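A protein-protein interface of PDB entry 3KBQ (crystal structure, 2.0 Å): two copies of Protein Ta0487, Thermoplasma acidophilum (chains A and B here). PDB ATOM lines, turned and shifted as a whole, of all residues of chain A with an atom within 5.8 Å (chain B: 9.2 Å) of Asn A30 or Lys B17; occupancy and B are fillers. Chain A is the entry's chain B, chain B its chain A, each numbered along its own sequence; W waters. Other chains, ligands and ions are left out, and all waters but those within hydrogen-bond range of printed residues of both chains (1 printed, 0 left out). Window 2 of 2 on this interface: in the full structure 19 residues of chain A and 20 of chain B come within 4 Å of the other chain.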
ATOM      1  N   ALA A  25      -1.934  10.129  21.748  1.00  0.00           N
ATOM      2  CA  ALA A  25      -2.525   9.202  20.779  1.00  0.00           C
ATOM      3  C   ALA A  25      -3.666   9.900  20.014  1.00  0.00           C
ATOM      4  O   ALA A  25      -3.847   9.674  18.827  1.00  0.00           O
ATOM      5  CB  ALA A  25      -3.020   7.885  21.478  1.00  0.00           C
ATOM      6  N   ALA A  26      -4.402  10.772  20.689  1.00  0.00           N
ATOM      7  CA  ALA A  26      -5.443  11.592  20.028  1.00  0.00           C
ATOM      8  C   ALA A  26      -4.835  12.516  19.011  1.00  0.00           C
ATOM      9  O   ALA A  26      -5.302  12.579  17.907  1.00  0.00           O
ATOM     10  CB  ALA A  26      -6.314  12.393  21.034  1.00  0.00           C
ATOM     11  N   PHE A  27      -3.809  13.252  19.396  1.00  0.00           N
ATOM     12  CA  PHE A  27      -3.175  14.187  18.467  1.00  0.00           C
ATOM     13  C   PHE A  27      -2.591  13.431  17.246  1.00  0.00           C
ATOM     14  O   PHE A  27      -2.789  13.844  16.103  1.00  0.00           O
ATOM     15  CB  PHE A  27      -2.077  14.992  19.164  1.00  0.00           C
ATOM     16  CG  PHE A  27      -1.347  15.952  18.231  1.00  0.00           C
ATOM     17  CD1 PHE A  27      -1.695  17.286  18.179  1.00  0.00           C
ATOM     18  CD2 PHE A  27      -0.294  15.516  17.429  1.00  0.00           C
ATOM     19  CE1 PHE A  27      -1.025  18.179  17.316  1.00  0.00           C
ATOM     20  CE2 PHE A  27       0.371  16.417  16.575  1.00  0.00           C
ATOM     21  CZ  PHE A  27      -0.019  17.727  16.523  1.00  0.00           C
ATOM     22  N   ILE A  28      -1.935  12.297  17.486  1.00  0.00           N
ATOM     23  CA  ILE A  28      -1.344  11.518  16.373  1.00  0.00           C
ATOM     24  C   ILE A  28      -2.460  10.932  15.491  1.00  0.00           C
ATOM     25  O   ILE A  28      -2.401  11.002  14.257  1.00  0.00           O
ATOM     26  CB  ILE A  28      -0.381  10.408  16.910  1.00  0.00           C
ATOM     27  CG1 ILE A  28       0.852  11.037  17.626  1.00  0.00           C
ATOM     28  CG2 ILE A  28       0.043   9.409  15.755  1.00  0.00           C
ATOM     29  CD1 ILE A  28       1.648  10.011  18.559  1.00  0.00           C
ATOM     30  N   GLY A  29      -3.495  10.374  16.125  1.00  0.00           N
ATOM     31  CA  GLY A  29      -4.628   9.827  15.384  1.00  0.00           C
ATOM     32  C   GLY A  29      -5.268  10.869  14.481  1.00  0.00           C
ATOM     33  O   GLY A  29      -5.576  10.587  13.317  1.00  0.00           O
ATOM     34  N   ASN A  30      -5.448  12.077  15.024  1.00  0.00           N
ATOM     35  CA  ASN A  30      -6.059  13.152  14.262  1.00  0.00           C
ATOM     36  C   ASN A  30      -5.130  13.631  13.132  1.00  0.00           C
ATOM     37  O   ASN A  30      -5.593  13.849  12.006  1.00  0.00           O
ATOM     38  CB  ASN A  30      -6.449  14.328  15.183  1.00  0.00           C
ATOM     39  CG  ASN A  30      -7.128  15.462  14.409  1.00  0.00           C
ATOM     40  OD1 ASN A  30      -8.207  15.294  13.846  1.00  0.00           O
ATOM     41  ND2 ASN A  30      -6.481  16.592  14.357  1.00  0.00           N
ATOM     42  N   PHE A  31      -3.829  13.758  13.426  1.00  0.00           N
ATOM     43  CA  PHE A  31      -2.826  14.182  12.439  1.00  0.00           C
ATOM     44  C   PHE A  31      -2.813  13.207  11.266  1.00  0.00           C
ATOM     45  O   PHE A  31      -2.860  13.636  10.124  1.00  0.00           O
ATOM     46  CB  PHE A  31      -1.441  14.293  13.087  1.00  0.00           C
ATOM     47  CG  PHE A  31      -0.323  14.712  12.128  1.00  0.00           C
ATOM     48  CD1 PHE A  31       0.007  16.051  11.968  1.00  0.00           C
ATOM     49  CD2 PHE A  31       0.426  13.756  11.441  1.00  0.00           C
ATOM     50  CE1 PHE A  31       1.052  16.443  11.082  1.00  0.00           C
ATOM     51  CE2 PHE A  31       1.474  14.148  10.556  1.00  0.00           C
ATOM     52  CZ  PHE A  31       1.767  15.495  10.391  1.00  0.00           C
ATOM     53  N   LEU A  32      -2.796  11.903  11.568  1.00  0.00           N
ATOM     54  CA  LEU A  32      -2.727  10.876  10.509  1.00  0.00           C
ATOM     55  C   LEU A  32      -4.026  10.832   9.691  1.00  0.00           C
ATOM     56  O   LEU A  32      -3.973  10.769   8.455  1.00  0.00           O
ATOM     57  CB  LEU A  32      -2.447   9.495  11.097  1.00  0.00           C
ATOM     58  CG  LEU A  32      -1.091   9.412  11.822  1.00  0.00           C
ATOM     59  CD1 LEU A  32      -0.980   8.116  12.579  1.00  0.00           C
ATOM     60  CD2 LEU A  32      -0.011   9.569  10.756  1.00  0.00           C
ATOM     61  N   THR A  33      -5.158  10.852  10.391  1.00  0.00           N
ATOM     62  CA  THR A  33      -6.488  10.963   9.754  1.00  0.00           C
ATOM     63  C   THR A  33      -6.574  12.160   8.821  1.00  0.00           C
ATOM     64  O   THR A  33      -7.078  12.053   7.666  1.00  0.00           O
ATOM     65  CB  THR A  33      -7.636  11.043  10.805  1.00  0.00           C
ATOM     66  OG1 THR A  33      -7.592   9.887  11.620  1.00  0.00           O
ATOM     67  CG2 THR A  33      -9.073  11.085  10.125  1.00  0.00           C
ATOM     68  N   TYR A  34      -6.106  13.297   9.315  1.00  0.00           N
ATOM     69  CA  TYR A  34      -6.090  14.522   8.557  1.00  0.00           C
ATOM     70  C   TYR A  34      -5.301  14.335   7.262  1.00  0.00           C
ATOM     71  O   TYR A  34      -5.691  14.898   6.236  1.00  0.00           O
ATOM     72  CB  TYR A  34      -5.455  15.666   9.354  1.00  0.00           C
ATOM     73  CG  TYR A  34      -5.535  17.041   8.687  1.00  0.00           C
ATOM     74  CD1 TYR A  34      -6.695  17.835   8.775  1.00  0.00           C
ATOM     75  CD2 TYR A  34      -4.442  17.549   7.976  1.00  0.00           C
ATOM     76  CE1 TYR A  34      -6.755  19.118   8.160  1.00  0.00           C
ATOM     77  CE2 TYR A  34      -4.507  18.814   7.317  1.00  0.00           C
ATOM     78  CZ  TYR A  34      -5.645  19.586   7.438  1.00  0.00           C
ATOM     79  OH  TYR A  34      -5.654  20.827   6.842  1.00  0.00           O
ATOM     80  N   HIS A  35      -4.232  13.526   7.285  1.00  0.00           N
ATOM     81  CA  HIS A  35      -3.449  13.331   6.041  1.00  0.00           C
ATOM     82  C   HIS A  35      -3.887  12.130   5.228  1.00  0.00           C
ATOM     83  O   HIS A  35      -3.172  11.687   4.353  1.00  0.00           O
ATOM     84  CB  HIS A  35      -1.959  13.288   6.330  1.00  0.00           C
ATOM     85  CG  HIS A  35      -1.417  14.604   6.752  1.00  0.00           C
ATOM     86  ND1 HIS A  35      -1.286  14.960   8.079  1.00  0.00           N
ATOM     87  CD2 HIS A  35      -0.977  15.658   6.030  1.00  0.00           C
ATOM     88  CE1 HIS A  35      -0.776  16.177   8.152  1.00  0.00           C
ATOM     89  NE2 HIS A  35      -0.594  16.629   6.926  1.00  0.00           N
ATOM     90  N   GLN A  38      -5.807   5.665   7.224  1.00  0.00           N
ATOM     91  CA  GLN A  38      -6.685   4.940   8.119  1.00  0.00           C
ATOM     92  C   GLN A  38      -5.927   4.482   9.378  1.00  0.00           C
ATOM     93  O   GLN A  38      -4.976   3.674   9.309  1.00  0.00           O
ATOM     94  CB  GLN A  38      -7.367   3.736   7.418  1.00  0.00           C
ATOM     95  CG  GLN A  38      -8.141   2.872   8.469  1.00  0.00           C
ATOM     96  CD  GLN A  38      -8.966   1.768   7.867  1.00  0.00           C
ATOM     97  OE1 GLN A  38      -8.425   0.738   7.409  1.00  0.00           O
ATOM     98  NE2 GLN A  38     -10.294   1.936   7.901  1.00  0.00           N
ATOM     99  N   VAL A  39      -6.315   5.001  10.544  1.00  0.00           N
ATOM    100  CA  VAL A  39      -5.612   4.589  11.749  1.00  0.00           C
ATOM    101  C   VAL A  39      -6.218   3.248  12.209  1.00  0.00           C
ATOM    102  O   VAL A  39      -7.366   3.143  12.630  1.00  0.00           O
ATOM    103  CB  VAL A  39      -5.680   5.648  12.863  1.00  0.00           C
ATOM    104  CG1 VAL A  39      -4.875   5.182  14.114  1.00  0.00           C
ATOM    105  CG2 VAL A  39      -5.180   6.993  12.318  1.00  0.00           C
ATOM    106  N   GLY B  12     -13.481   1.432  19.233  1.00  0.00           N
ATOM    107  CA  GLY B  12     -14.142   2.621  18.677  1.00  0.00           C
ATOM    108  C   GLY B  12     -13.225   3.369  17.717  1.00  0.00           C
ATOM    109  O   GLY B  12     -12.146   3.822  18.098  1.00  0.00           O
ATOM    110  N   ASN B  13     -13.670   3.526  16.478  1.00  0.00           N
ATOM    111  CA  ASN B  13     -12.966   4.322  15.472  1.00  0.00           C
ATOM    112  C   ASN B  13     -12.713   5.751  15.915  1.00  0.00           C
ATOM    113  O   ASN B  13     -11.687   6.339  15.547  1.00  0.00           O
ATOM    114  CB  ASN B  13     -13.753   4.333  14.131  1.00  0.00           C
ATOM    115  CG  ASN B  13     -14.062   2.930  13.602  1.00  0.00           C
ATOM    116  OD1 ASN B  13     -13.445   1.942  13.973  1.00  0.00           O
ATOM    117  ND2 ASN B  13     -15.039   2.850  12.716  1.00  0.00           N
ATOM    118  N   GLU B  14     -13.640   6.324  16.697  1.00  0.00           N
ATOM    119  CA  GLU B  14     -13.504   7.734  17.115  1.00  0.00           C
ATOM    120  C   GLU B  14     -12.265   7.964  18.065  1.00  0.00           C
ATOM    121  O   GLU B  14     -11.652   9.042  18.081  1.00  0.00           O
ATOM    122  CB  GLU B  14     -14.811   8.218  17.764  1.00  0.00           C
ATOM    123  CG  GLU B  14     -15.056   7.724  19.222  1.00  0.00           C
ATOM    124  CD  GLU B  14     -15.630   6.290  19.343  1.00  0.00           C
ATOM    125  OE1 GLU B  14     -15.666   5.492  18.342  1.00  0.00           O
ATOM    126  OE2 GLU B  14     -16.074   5.969  20.484  1.00  0.00           O
ATOM    127  N   ILE B  15     -11.939   6.950  18.856  1.00  0.00           N
ATOM    128  CA  ILE B  15     -10.728   6.946  19.667  1.00  0.00           C
ATOM    129  C   ILE B  15      -9.459   6.884  18.816  1.00  0.00           C
ATOM    130  O   ILE B  15      -8.562   7.715  18.951  1.00  0.00           O
ATOM    131  CB  ILE B  15     -10.749   5.798  20.722  1.00  0.00           C
ATOM    132  CG1 ILE B  15     -12.000   5.866  21.618  1.00  0.00           C
ATOM    133  CG2 ILE B  15      -9.446   5.821  21.577  1.00  0.00           C
ATOM    134  CD1 ILE B  15     -12.028   7.062  22.592  1.00  0.00           C
ATOM    135  N   LEU B  16      -9.387   5.930  17.902  1.00  0.00           N
ATOM    136  CA  LEU B  16      -8.236   5.820  16.984  1.00  0.00           C
ATOM    137  C   LEU B  16      -8.004   7.077  16.183  1.00  0.00           C
ATOM    138  O   LEU B  16      -6.843   7.446  15.942  1.00  0.00           O
ATOM    139  CB  LEU B  16      -8.477   4.694  15.980  1.00  0.00           C
ATOM    140  CG  LEU B  16      -8.460   3.347  16.702  1.00  0.00           C
ATOM    141  CD1 LEU B  16      -9.177   2.332  15.802  1.00  0.00           C
ATOM    142  CD2 LEU B  16      -7.019   2.879  17.001  1.00  0.00           C
ATOM    143  N   LYS B  17      -9.083   7.718  15.731  1.00  0.00           N
ATOM    144  CA  LYS B  17      -8.924   8.904  14.888  1.00  0.00           C
ATOM    145  C   LYS B  17      -8.661  10.138  15.704  1.00  0.00           C
ATOM    146  O   LYS B  17      -8.470  11.216  15.142  1.00  0.00           O
ATOM    147  CB  LYS B  17     -10.120   9.133  13.949  1.00  0.00           C
ATOM    148  CG  LYS B  17     -10.237   7.969  12.952  1.00  0.00           C
ATOM    149  CD  LYS B  17     -11.531   8.008  12.161  1.00  0.00           C
ATOM    150  CE  LYS B  17     -12.017   6.609  11.864  1.00  0.00           C
ATOM    151  NZ  LYS B  17     -11.445   6.086  10.573  1.00  0.00           N
ATOM    152  N   GLY B  18      -8.658   9.980  17.030  1.00  0.00           N
ATOM    153  CA  GLY B  18      -8.455  11.125  17.930  1.00  0.00           C
ATOM    154  C   GLY B  18      -9.560  12.147  17.951  1.00  0.00           C
ATOM    155  O   GLY B  18      -9.288  13.331  18.144  1.00  0.00           O
ATOM    156  N   ARG B  19     -10.809  11.722  17.705  1.00  0.00           N
ATOM    157  CA  ARG B  19     -11.965  12.633  17.798  1.00  0.00           C
ATOM    158  C   ARG B  19     -12.241  12.874  19.264  1.00  0.00           C
ATOM    159  O   ARG B  19     -12.701  13.950  19.651  1.00  0.00           O
ATOM    160  CB  ARG B  19     -13.236  12.011  17.226  1.00  0.00           C
ATOM    161  CG  ARG B  19     -13.125  11.527  15.816  1.00  0.00           C
ATOM    162  CD  ARG B  19     -13.366  12.620  14.784  1.00  0.00           C
ATOM    163  NE  ARG B  19     -14.504  13.498  15.098  1.00  0.00           N
ATOM    164  CZ  ARG B  19     -15.014  14.405  14.257  1.00  0.00           C
ATOM    165  NH1 ARG B  19     -14.517  14.530  13.030  1.00  0.00           N
ATOM    166  NH2 ARG B  19     -16.034  15.184  14.629  1.00  0.00           N
ATOM    167  N   THR B  20     -12.005  11.826  20.044  1.00  0.00           N
ATOM    168  CA  THR B  20     -12.321  11.759  21.463  1.00  0.00           C
ATOM    169  C   THR B  20     -11.056  11.266  22.186  1.00  0.00           C
ATOM    170  O   THR B  20     -10.420  10.286  21.780  1.00  0.00           O
ATOM    171  CB  THR B  20     -13.464  10.724  21.693  1.00  0.00           C
ATOM    172  OG1 THR B  20     -14.665  11.198  21.044  1.00  0.00           O
ATOM    173  CG2 THR B  20     -13.753  10.488  23.200  1.00  0.00           C
ATOM    174  N   VAL B  21     -10.679  11.944  23.246  1.00  0.00           N
ATOM    175  CA  VAL B  21      -9.551  11.482  24.046  1.00  0.00           C
ATOM    176  C   VAL B  21      -9.976  10.223  24.810  1.00  0.00           C
ATOM    177  O   VAL B  21     -11.117  10.132  25.273  1.00  0.00           O
ATOM    178  CB  VAL B  21      -9.172  12.597  25.065  1.00  0.00           C
ATOM    179  CG1 VAL B  21      -7.996  12.160  25.924  1.00  0.00           C
ATOM    180  CG2 VAL B  21      -8.808  13.870  24.312  1.00  0.00           C
ATOM    181  N   VAL B  44      -6.270  -0.522  21.290  1.00  0.00           N
ATOM    182  CA  VAL B  44      -7.351   0.272  20.815  1.00  0.00           C
ATOM    183  C   VAL B  44      -7.666  -0.295  19.419  1.00  0.00           C
ATOM    184  O   VAL B  44      -6.765  -0.407  18.610  1.00  0.00           O
ATOM    185  CB  VAL B  44      -7.007   1.799  20.732  1.00  0.00           C
ATOM    186  CG1 VAL B  44      -8.233   2.545  20.280  1.00  0.00           C
ATOM    187  CG2 VAL B  44      -6.642   2.346  22.082  1.00  0.00           C
ATOM    188  N   VAL B  45      -8.910  -0.689  19.163  1.00  0.00           N
ATOM    189  CA  VAL B  45      -9.244  -1.296  17.872  1.00  0.00           C
ATOM    190  C   VAL B  45     -10.471  -0.686  17.268  1.00  0.00           C
ATOM    191  O   VAL B  45     -11.268   0.000  17.960  1.00  0.00           O
ATOM    192  CB  VAL B  45      -9.444  -2.886  17.942  1.00  0.00           C
ATOM    193  CG1 VAL B  45      -8.093  -3.567  18.166  1.00  0.00           C
ATOM    194  CG2 VAL B  45     -10.493  -3.272  19.029  1.00  0.00           C
ATOM    195  N   MET B  46     -10.608  -0.906  15.968  1.00  0.00           N
ATOM    196  CA  MET B  46     -11.778  -0.484  15.211  1.00  0.00           C
ATOM    197  C   MET B  46     -12.993  -1.297  15.598  1.00  0.00           C
ATOM    198  O   MET B  46     -12.882  -2.398  16.183  1.00  0.00           O
ATOM    199  CB  MET B  46     -11.521  -0.661  13.710  1.00  0.00           C
ATOM    200  CG  MET B  46     -10.504   0.416  13.138  1.00  0.00           C
ATOM    201  SD  MET B  46     -10.076   0.232  11.357  1.00  0.00           S
ATOM    202  CE  MET B  46      -9.992  -1.465  11.167  1.00  0.00           C
ATOM    203  N   ASP B  47     -14.157  -0.765  15.241  1.00  0.00           N
ATOM    204  CA  ASP B  47     -15.428  -1.466  15.376  1.00  0.00           C
ATOM    205  C   ASP B  47     -15.527  -2.528  14.287  1.00  0.00           C
ATOM    206  O   ASP B  47     -16.234  -2.340  13.299  1.00  0.00           O
ATOM    207  CB  ASP B  47     -16.578  -0.485  15.220  1.00  0.00           C
ATOM    208  CG  ASP B  47     -16.536   0.613  16.251  1.00  0.00           C
ATOM    209  OD1 ASP B  47     -16.628   0.306  17.470  1.00  0.00           O
ATOM    210  OD2 ASP B  47     -16.420   1.785  15.851  1.00  0.00           O
HETATM  211  O   HOH W   1      -4.681   7.031  17.917  1.00  0.00           O
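No position is printed for both chains.
Ala A26 touches Gly B18 (O to CA, 3.5 Å).
Gly A29 touches Leu B16 (CA to O, 3.3 Å).
Thr A33 touches Lys B17.
Met B46 touches Gln A38 (SD to NE2, 3.9 Å).
Leu B16 touches Val A39.
Hydrophobic or aromatic side chains of chain A within 4 Å of the printed part of chain B: Ala A26 and Val A39.
Of the 14 printed residues of chain B, 4 touch a printed residue of chain A.
Hydrophobic or aromatic side chains of chain B within 4 Å of the printed part of chain A: Leu B16 and Met B46.
Among the printed residues, 7 pairs touch across the chains.
Among the printed residues, no Asp or Glu carboxylate lies within 4 Å of a Lys or Arg side-chain nitrogen of the other chain.
Gly A29 touches just these residues of chain B: Leu B16 (3.3 Å) and Lys B17 (3.3 Å).
Asn A30 touches one residue of chain B.
Thr A33 touches just one residue of chain B: Lys B17.
Of the printed residues of chain B, Val A39 touches Leu B16 (3.5 Å).
Of chain A, only Gly A29 (3.3 Å), Asn A30 (3.1 Å) and Thr A33 (3.5 Å) come within 4 Å of Lys B17.
Printed residues of chain A within 4 Å of Met B46: Gln A38 (3.9 Å).
The nearest residue of chain B that does not touch Asn A30 is Gly B18 (4.2 Å).
The nearest residue of chain A that does not touch Lys B17 is Ala A26 (4.4 Å).
The nearest printed residue of chain B that does not touch Gln A38 is Lys B17 (5.1 Å).
O of Gly A29 lies within hydrogen-bond range of OG1 of Thr A33, 2.7 Å away.
Water W1 lies within hydrogen-bond range of O of Ala A25 (2.9 Å) and O of Leu B16 (3.0 Å).
The backbone carbonyl oxygen (O) of Lys B17 is in hydrogen-bond range of the backbone NH (N) of Asn A30.
The backbone carbonyl oxygen (O) of Lys B17 lies close to the backbone carbonyl oxygen (O) of Gly A29, 3.5 Å away.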
